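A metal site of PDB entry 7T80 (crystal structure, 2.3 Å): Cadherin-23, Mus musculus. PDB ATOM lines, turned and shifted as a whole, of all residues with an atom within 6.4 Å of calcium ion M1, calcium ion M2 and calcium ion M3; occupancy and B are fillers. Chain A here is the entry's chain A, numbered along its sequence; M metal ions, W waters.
OD1 of Asp 109 sits close to ND2 of Asn 110 (3.0 Å).
N of Arg 71 lies close to OE1 of Glu 17.
The backbone NH of Glu 17 is in hydrogen-bond range of the backbone carbonyl oxygen of Ala 105, at 3.1 Å.
The side-chain carboxylate (OD1) of Asp 200 sits at hydrogen-bond distance from the backbone NH (N) of Leu 204 (3.0 Å).
The side-chain carboxylate (OE2) of Glu 72 lies close to the side-chain amide nitrogen (ND2) of Asn 110, at 3.2 Å.
OE1 of Glu 72 lies close to NH2 of Arg 71, at 2.9 Å.
The guanidinium group of Arg 71 lies close to the side-chain carboxylate of Asp 106 (3.1 Å).
The side-chain carboxylate (OD2) of Asp 106 sits at hydrogen-bond distance from the backbone NH (N) of Glu 147 (3.0 Å).
The nearest printed residue that does not touch calcium ion M1 is His 111 (4.4 Å).
Within 4 Å of calcium ion M2: Glu 17, Glu 72, Asp 106, Glu 107, Asp 109, Asn 110 and Asp 146.
Along chain A the residues within 4 Å of calcium ion M2 span positions 17 to 146.
Along chain A the residues within 4 Å of calcium ion M3 span positions 17 to 109.
The nearest printed residue that does not touch calcium ion M3 is Arg 71 (4.2 Å).
Calcium ion M1 is bound by OD2 of Asp 144 (2.3 Å), OD2 of Asp 200 (2.3 Å), O of Tyr 150 (2.3 Å), OD2 of Asp 146 (2.3 Å), OD1 of Asn 108 (2.4 Å), O of Asn 110 (2.4 Å) and OD1 of Asp 144 (2.6 Å).
Calcium ion M2 is bound by OE2 of Glu 17 (2.3 Å), OD1 of Asp 146 (2.3 Å), OD1 of Asp 106 (2.3 Å), O of Glu 107 (2.4 Å), OD1 of Asp 109 (2.4 Å), OE1 of Glu 72 (2.5 Å) and OE2 of Glu 72 (2.6 Å).
Calcium ion M3 is bound by the side-chain carboxylate (OD2) of Asp 109, the side-chain carboxylate (OD1) of Asp 70, the side-chain carboxylate (OE2) of Glu 72, water W2, the side-chain carboxylate (OE1) of Glu 17 and water W1.
Calcium ion M3 has six donor atoms within binding distance.
Slightly farther from calcium ion M3 lies OD1 of Asp 109 (3.1 Å).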
ATOM      1  N   GLU A  17      13.410   0.434  27.356  1.00  0.00           N
ATOM      2  CA  GLU A  17      14.268   1.647  27.299  1.00  0.00           C
ATOM      3  C   GLU A  17      13.604   2.760  26.483  1.00  0.00           C
ATOM      4  O   GLU A  17      14.054   3.878  26.649  1.00  0.00           O
ATOM      5  CB  GLU A  17      15.656   1.325  26.745  1.00  0.00           C
ATOM      6  CG  GLU A  17      15.681   0.905  25.291  1.00  0.00           C
ATOM      7  CD  GLU A  17      17.086   0.920  24.721  1.00  0.00           C
ATOM      8  OE1 GLU A  17      17.803   1.888  25.088  1.00  0.00           O
ATOM      9  OE2 GLU A  17      17.464  -0.020  23.948  1.00  0.00           O
ATOM     10  N   ASN A  18      12.567   2.491  25.677  1.00  0.00           N
ATOM     11  CA  ASN A  18      11.867   3.544  24.902  1.00  0.00           C
ATOM     12  C   ASN A  18      10.626   4.081  25.646  1.00  0.00           C
ATOM     13  O   ASN A  18       9.939   4.948  25.054  1.00  0.00           O
ATOM     14  CB  ASN A  18      11.476   3.068  23.503  1.00  0.00           C
ATOM     15  CG  ASN A  18      12.687   2.876  22.625  1.00  0.00           C
ATOM     16  OD1 ASN A  18      13.811   3.165  23.034  1.00  0.00           O
ATOM     17  ND2 ASN A  18      12.474   2.351  21.439  1.00  0.00           N
ATOM     18  N   LEU A  69      15.281   7.534  28.574  1.00  0.00           N
ATOM     19  CA  LEU A  69      16.099   6.430  29.113  1.00  0.00           C
ATOM     20  C   LEU A  69      16.927   5.841  27.971  1.00  0.00           C
ATOM     21  O   LEU A  69      16.545   6.053  26.828  1.00  0.00           O
ATOM     22  CB  LEU A  69      15.170   5.372  29.699  1.00  0.00           C
ATOM     23  CG  LEU A  69      14.188   5.864  30.751  1.00  0.00           C
ATOM     24  CD1 LEU A  69      13.364   4.724  31.321  1.00  0.00           C
ATOM     25  CD2 LEU A  69      14.906   6.568  31.877  1.00  0.00           C
ATOM     26  N   ASP A  70      17.992   5.112  28.298  1.00  0.00           N
ATOM     27  CA  ASP A  70      18.932   4.533  27.308  1.00  0.00           C
ATOM     28  C   ASP A  70      19.620   3.325  27.948  1.00  0.00           C
ATOM     29  O   ASP A  70      20.477   3.534  28.821  1.00  0.00           O
ATOM     30  CB  ASP A  70      19.929   5.590  26.834  1.00  0.00           C
ATOM     31  CG  ASP A  70      20.767   5.123  25.648  1.00  0.00           C
ATOM     32  OD1 ASP A  70      20.509   3.994  25.140  1.00  0.00           O
ATOM     33  OD2 ASP A  70      21.662   5.878  25.235  1.00  0.00           O
ATOM     34  N   ARG A  71      19.207   2.117  27.577  1.00  0.00           N
ATOM     35  CA  ARG A  71      19.789   0.889  28.157  1.00  0.00           C
ATOM     36  C   ARG A  71      21.305   0.938  27.947  1.00  0.00           C
ATOM     37  O   ARG A  71      22.030   0.444  28.812  1.00  0.00           O
ATOM     38  CB  ARG A  71      19.210  -0.356  27.503  1.00  0.00           C
ATOM     39  CG  ARG A  71      19.527  -1.648  28.247  1.00  0.00           C
ATOM     40  CD  ARG A  71      19.534  -2.875  27.321  1.00  0.00           C
ATOM     41  NE  ARG A  71      20.559  -2.695  26.301  1.00  0.00           N
ATOM     42  CZ  ARG A  71      21.857  -2.873  26.513  1.00  0.00           C
ATOM     43  NH1 ARG A  71      22.306  -3.325  27.680  1.00  0.00           N
ATOM     44  NH2 ARG A  71      22.692  -2.663  25.527  1.00  0.00           N
ATOM     45  N   GLU A  72      21.735   1.506  26.813  1.00  0.00           N
ATOM     46  CA  GLU A  72      23.155   1.601  26.377  1.00  0.00           C
ATOM     47  C   GLU A  72      23.930   2.566  27.276  1.00  0.00           C
ATOM     48  O   GLU A  72      25.157   2.499  27.243  1.00  0.00           O
ATOM     49  CB  GLU A  72      23.229   2.060  24.917  1.00  0.00           C
ATOM     50  CG  GLU A  72      22.943   0.936  23.942  1.00  0.00           C
ATOM     51  CD  GLU A  72      21.506   0.433  23.790  1.00  0.00           C
ATOM     52  OE1 GLU A  72      21.333  -0.793  23.850  1.00  0.00           O
ATOM     53  OE2 GLU A  72      20.570   1.233  23.489  1.00  0.00           O
ATOM     54  N   ARG A  73      23.243   3.455  28.022  1.00  0.00           N
ATOM     55  CA  ARG A  73      23.896   4.471  28.884  1.00  0.00           C
ATOM     56  C   ARG A  73      23.803   4.017  30.343  1.00  0.00           C
ATOM     57  O   ARG A  73      24.858   3.808  30.954  1.00  0.00           O
ATOM     58  CB  ARG A  73      23.268   5.857  28.689  1.00  0.00           C
ATOM     59  CG  ARG A  73      24.261   7.010  28.815  1.00  0.00           C
ATOM     60  CD  ARG A  73      23.666   8.328  28.327  1.00  0.00           C
ATOM     61  NE  ARG A  73      22.791   8.795  29.382  1.00  0.00           N
ATOM     62  CZ  ARG A  73      23.189   9.444  30.468  1.00  0.00           C
ATOM     63  NH1 ARG A  73      22.315   9.768  31.402  1.00  0.00           N
ATOM     64  NH2 ARG A  73      24.463   9.774  30.631  1.00  0.00           N
ATOM     65  N   ALA A 105      14.661  -3.101  29.411  1.00  0.00           N
ATOM     66  CA  ALA A 105      14.648  -4.121  28.339  1.00  0.00           C
ATOM     67  C   ALA A 105      15.195  -3.459  27.079  1.00  0.00           C
ATOM     68  O   ALA A 105      14.847  -2.292  26.809  1.00  0.00           O
ATOM     69  CB  ALA A 105      13.253  -4.627  28.106  1.00  0.00           C
ATOM     70  N   ASP A 106      15.999  -4.199  26.329  1.00  0.00           N
ATOM     71  CA  ASP A 106      16.714  -3.687  25.142  1.00  0.00           C
ATOM     72  C   ASP A 106      15.736  -3.480  23.990  1.00  0.00           C
ATOM     73  O   ASP A 106      15.062  -4.435  23.621  1.00  0.00           O
ATOM     74  CB  ASP A 106      17.805  -4.661  24.695  1.00  0.00           C
ATOM     75  CG  ASP A 106      18.695  -4.050  23.611  1.00  0.00           C
ATOM     76  OD1 ASP A 106      18.988  -2.820  23.681  1.00  0.00           O
ATOM     77  OD2 ASP A 106      19.068  -4.804  22.707  1.00  0.00           O
ATOM     78  N   GLU A 107      15.721  -2.282  23.416  1.00  0.00           N
ATOM     79  CA  GLU A 107      15.073  -1.998  22.111  1.00  0.00           C
ATOM     80  C   GLU A 107      16.163  -1.940  21.026  1.00  0.00           C
ATOM     81  O   GLU A 107      17.352  -1.604  21.320  1.00  0.00           O
ATOM     82  CB  GLU A 107      14.239  -0.714  22.157  1.00  0.00           C
ATOM     83  CG  GLU A 107      13.056  -0.747  23.103  1.00  0.00           C
ATOM     84  CD  GLU A 107      12.008  -1.804  22.800  1.00  0.00           C
ATOM     85  OE1 GLU A 107      11.914  -2.211  21.634  1.00  0.00           O
ATOM     86  OE2 GLU A 107      11.287  -2.236  23.727  1.00  0.00           O
ATOM     87  N   ASN A 108      15.781  -2.309  19.811  1.00  0.00           N
ATOM     88  CA  ASN A 108      16.674  -2.273  18.636  1.00  0.00           C
ATOM     89  C   ASN A 108      16.807  -0.827  18.158  1.00  0.00           C
ATOM     90  O   ASN A 108      16.202  -0.539  17.154  1.00  0.00           O
ATOM     91  CB  ASN A 108      16.138  -3.165  17.499  1.00  0.00           C
ATOM     92  CG  ASN A 108      17.211  -3.525  16.510  1.00  0.00           C
ATOM     93  OD1 ASN A 108      18.382  -3.571  16.858  1.00  0.00           O
ATOM     94  ND2 ASN A 108      16.841  -3.803  15.273  1.00  0.00           N
ATOM     95  N   ASP A 109      17.540   0.028  18.869  1.00  0.00           N
ATOM     96  CA  ASP A 109      17.669   1.474  18.517  1.00  0.00           C
ATOM     97  C   ASP A 109      19.092   1.747  18.002  1.00  0.00           C
ATOM     98  O   ASP A 109      19.452   2.924  17.839  1.00  0.00           O
ATOM     99  CB  ASP A 109      17.280   2.411  19.680  1.00  0.00           C
ATOM    100  CG  ASP A 109      17.929   2.134  21.029  1.00  0.00           C
ATOM    101  OD1 ASP A 109      18.593   1.113  21.146  1.00  0.00           O
ATOM    102  OD2 ASP A 109      17.735   2.959  21.985  1.00  0.00           O
ATOM    103  N   ASN A 110      19.888   0.723  17.761  1.00  0.00           N
ATOM    104  CA  ASN A 110      21.258   0.899  17.219  1.00  0.00           C
ATOM    105  C   ASN A 110      21.433   0.008  15.997  1.00  0.00           C
ATOM    106  O   ASN A 110      20.796  -1.068  15.921  1.00  0.00           O
ATOM    107  CB  ASN A 110      22.352   0.601  18.248  1.00  0.00           C
ATOM    108  CG  ASN A 110      22.318   1.566  19.414  1.00  0.00           C
ATOM    109  OD1 ASN A 110      23.023   2.568  19.410  1.00  0.00           O
ATOM    110  ND2 ASN A 110      21.500   1.251  20.411  1.00  0.00           N
ATOM    111  N   HIS A 111      22.267   0.440  15.061  1.00  0.00           N
ATOM    112  CA  HIS A 111      22.559  -0.306  13.813  1.00  0.00           C
ATOM    113  C   HIS A 111      24.037  -0.626  13.755  1.00  0.00           C
ATOM    114  O   HIS A 111      24.850   0.033  14.422  1.00  0.00           O
ATOM    115  CB  HIS A 111      22.016   0.440  12.574  1.00  0.00           C
ATOM    116  CG  HIS A 111      22.639   1.773  12.352  1.00  0.00           C
ATOM    117  ND1 HIS A 111      23.787   1.934  11.560  1.00  0.00           N
ATOM    118  CD2 HIS A 111      22.285   2.996  12.797  1.00  0.00           C
ATOM    119  CE1 HIS A 111      24.104   3.211  11.542  1.00  0.00           C
ATOM    120  NE2 HIS A 111      23.203   3.886  12.293  1.00  0.00           N
ATOM    121  N   PRO A 112      24.408  -1.682  13.007  1.00  0.00           N
ATOM    122  CA  PRO A 112      25.810  -2.035  12.814  1.00  0.00           C
ATOM    123  C   PRO A 112      26.583  -0.857  12.197  1.00  0.00           C
ATOM    124  O   PRO A 112      26.114  -0.286  11.258  1.00  0.00           O
ATOM    125  CB  PRO A 112      25.754  -3.228  11.861  1.00  0.00           C
ATOM    126  CG  PRO A 112      24.335  -3.756  11.988  1.00  0.00           C
ATOM    127  CD  PRO A 112      23.494  -2.527  12.227  1.00  0.00           C
ATOM    128  N   ASP A 144      27.375  -3.512  16.719  1.00  0.00           N
ATOM    129  CA  ASP A 144      26.011  -3.023  17.056  1.00  0.00           C
ATOM    130  C   ASP A 144      25.959  -2.935  18.579  1.00  0.00           C
ATOM    131  O   ASP A 144      26.106  -3.995  19.232  1.00  0.00           O
ATOM    132  CB  ASP A 144      24.947  -3.880  16.373  1.00  0.00           C
ATOM    133  CG  ASP A 144      23.501  -3.409  16.536  1.00  0.00           C
ATOM    134  OD1 ASP A 144      23.080  -3.188  17.695  1.00  0.00           O
ATOM    135  OD2 ASP A 144      22.760  -3.358  15.526  1.00  0.00           O
ATOM    136  N   ALA A 145      25.714  -1.718  19.096  1.00  0.00           N
ATOM    137  CA  ALA A 145      25.698  -1.355  20.522  1.00  0.00           C
ATOM    138  C   ALA A 145      24.506  -1.979  21.276  1.00  0.00           C
ATOM    139  O   ALA A 145      24.453  -1.801  22.479  1.00  0.00           O
ATOM    140  CB  ALA A 145      25.665   0.154  20.650  1.00  0.00           C
ATOM    141  N   ASP A 146      23.581  -2.677  20.638  1.00  0.00           N
ATOM    142  CA  ASP A 146      22.412  -3.247  21.379  1.00  0.00           C
ATOM    143  C   ASP A 146      22.918  -4.418  22.244  1.00  0.00           C
ATOM    144  O   ASP A 146      24.136  -4.661  22.226  1.00  0.00           O
ATOM    145  CB  ASP A 146      21.285  -3.569  20.409  1.00  0.00           C
ATOM    146  CG  ASP A 146      20.603  -2.323  19.877  1.00  0.00           C
ATOM    147  OD1 ASP A 146      20.200  -1.481  20.732  1.00  0.00           O
ATOM    148  OD2 ASP A 146      20.465  -2.223  18.618  1.00  0.00           O
ATOM    149  N   GLU A 147      22.049  -5.064  23.012  1.00  0.00           N
ATOM    150  CA  GLU A 147      22.447  -5.913  24.172  1.00  0.00           C
ATOM    151  C   GLU A 147      22.976  -7.273  23.700  1.00  0.00           C
ATOM    152  O   GLU A 147      24.127  -7.584  24.044  1.00  0.00           O
ATOM    153  CB  GLU A 147      21.290  -6.095  25.157  1.00  0.00           C
ATOM    154  CG  GLU A 147      21.602  -7.101  26.267  1.00  0.00           C
ATOM    155  CD  GLU A 147      20.706  -6.968  27.486  1.00  0.00           C
ATOM    156  OE1 GLU A 147      19.481  -6.781  27.326  1.00  0.00           O
ATOM    157  OE2 GLU A 147      21.249  -7.022  28.601  1.00  0.00           O
ATOM    158  N   TYR A 150      19.669  -8.220  19.421  1.00  0.00           N
ATOM    159  CA  TYR A 150      19.542  -7.056  18.518  1.00  0.00           C
ATOM    160  C   TYR A 150      20.923  -6.553  18.083  1.00  0.00           C
ATOM    161  O   TYR A 150      21.007  -5.511  17.458  1.00  0.00           O
ATOM    162  CB  TYR A 150      18.701  -5.992  19.231  1.00  0.00           C
ATOM    163  CG  TYR A 150      17.243  -6.330  19.363  1.00  0.00           C
ATOM    164  CD1 TYR A 150      16.561  -6.916  18.311  1.00  0.00           C
ATOM    165  CD2 TYR A 150      16.528  -6.005  20.505  1.00  0.00           C
ATOM    166  CE1 TYR A 150      15.206  -7.170  18.386  1.00  0.00           C
ATOM    167  CE2 TYR A 150      15.168  -6.278  20.605  1.00  0.00           C
ATOM    168  CZ  TYR A 150      14.515  -6.870  19.553  1.00  0.00           C
ATOM    169  OH  TYR A 150      13.172  -7.163  19.606  1.00  0.00           O
ATOM    170  N   ALA A 151      21.996  -7.239  18.467  1.00  0.00           N
ATOM    171  CA  ALA A 151      23.383  -6.828  18.172  1.00  0.00           C
ATOM    172  C   ALA A 151      24.076  -7.883  17.308  1.00  0.00           C
ATOM    173  O   ALA A 151      25.219  -7.610  16.880  1.00  0.00           O
ATOM    174  CB  ALA A 151      24.112  -6.588  19.475  1.00  0.00           C
ATOM    175  N   VAL A 152      23.454  -9.043  17.059  1.00  0.00           N
ATOM    176  CA  VAL A 152      24.024 -10.059  16.132  1.00  0.00           C
ATOM    177  C   VAL A 152      24.026  -9.461  14.721  1.00  0.00           C
ATOM    178  O   VAL A 152      22.972  -9.016  14.240  1.00  0.00           O
ATOM    179  CB  VAL A 152      23.304 -11.431  16.184  1.00  0.00           C
ATOM    180  CG1 VAL A 152      23.845 -12.366  15.101  1.00  0.00           C
ATOM    181  CG2 VAL A 152      23.446 -12.072  17.564  1.00  0.00           C
ATOM    182  N   ASP A 200      21.378  -6.223  11.297  1.00  0.00           N
ATOM    183  CA  ASP A 200      20.910  -6.858  12.553  1.00  0.00           C
ATOM    184  C   ASP A 200      19.597  -7.551  12.215  1.00  0.00           C
ATOM    185  O   ASP A 200      19.168  -7.455  11.062  1.00  0.00           O
ATOM    186  CB  ASP A 200      20.895  -5.857  13.700  1.00  0.00           C
ATOM    187  CG  ASP A 200      19.776  -4.838  13.695  1.00  0.00           C
ATOM    188  OD1 ASP A 200      18.818  -4.992  12.882  1.00  0.00           O
ATOM    189  OD2 ASP A 200      19.849  -3.895  14.515  1.00  0.00           O
ATOM    190  N   ILE A 201      18.981  -8.235  13.177  1.00  0.00           N
ATOM    191  CA  ILE A 201      17.799  -9.112  12.940  1.00  0.00           C
ATOM    192  C   ILE A 201      16.543  -8.258  12.782  1.00  0.00           C
ATOM    193  O   ILE A 201      15.515  -8.800  12.353  1.00  0.00           O
ATOM    194  CB  ILE A 201      17.698 -10.166  14.077  1.00  0.00           C
ATOM    195  CG1 ILE A 201      16.900 -11.400  13.627  1.00  0.00           C
ATOM    196  CG2 ILE A 201      17.158  -9.554  15.372  1.00  0.00           C
ATOM    197  CD1 ILE A 201      17.629 -12.275  12.593  1.00  0.00           C
ATOM    198  N   LEU A 204      17.974  -3.374  10.479  1.00  0.00           N
ATOM    199  CA  LEU A 204      18.742  -2.092  10.530  1.00  0.00           C
ATOM    200  C   LEU A 204      20.146  -2.388   9.986  1.00  0.00           C
ATOM    201  O   LEU A 204      20.759  -3.328  10.430  1.00  0.00           O
ATOM    202  CB  LEU A 204      18.781  -1.537  11.960  1.00  0.00           C
ATOM    203  CG  LEU A 204      17.450  -1.219  12.646  1.00  0.00           C
ATOM    204  CD1 LEU A 204      17.678  -0.357  13.878  1.00  0.00           C
ATOM    205  CD2 LEU A 204      16.477  -0.518  11.717  1.00  0.00           C
HETATM  206 CA    CA M   1      20.717  -3.364  16.604  1.00  0.00          CA
HETATM  207 CA    CA M   2      19.150  -0.742  22.608  1.00  0.00          CA
HETATM  208 CA    CA M   3      19.150   3.081  23.500  1.00  0.00          CA
HETATM  209  O   HOH W   1      20.654   3.923  21.825  1.00  0.00           O
HETATM  210  O   HOH W   2      17.981   5.110  23.764  1.00  0.00           O
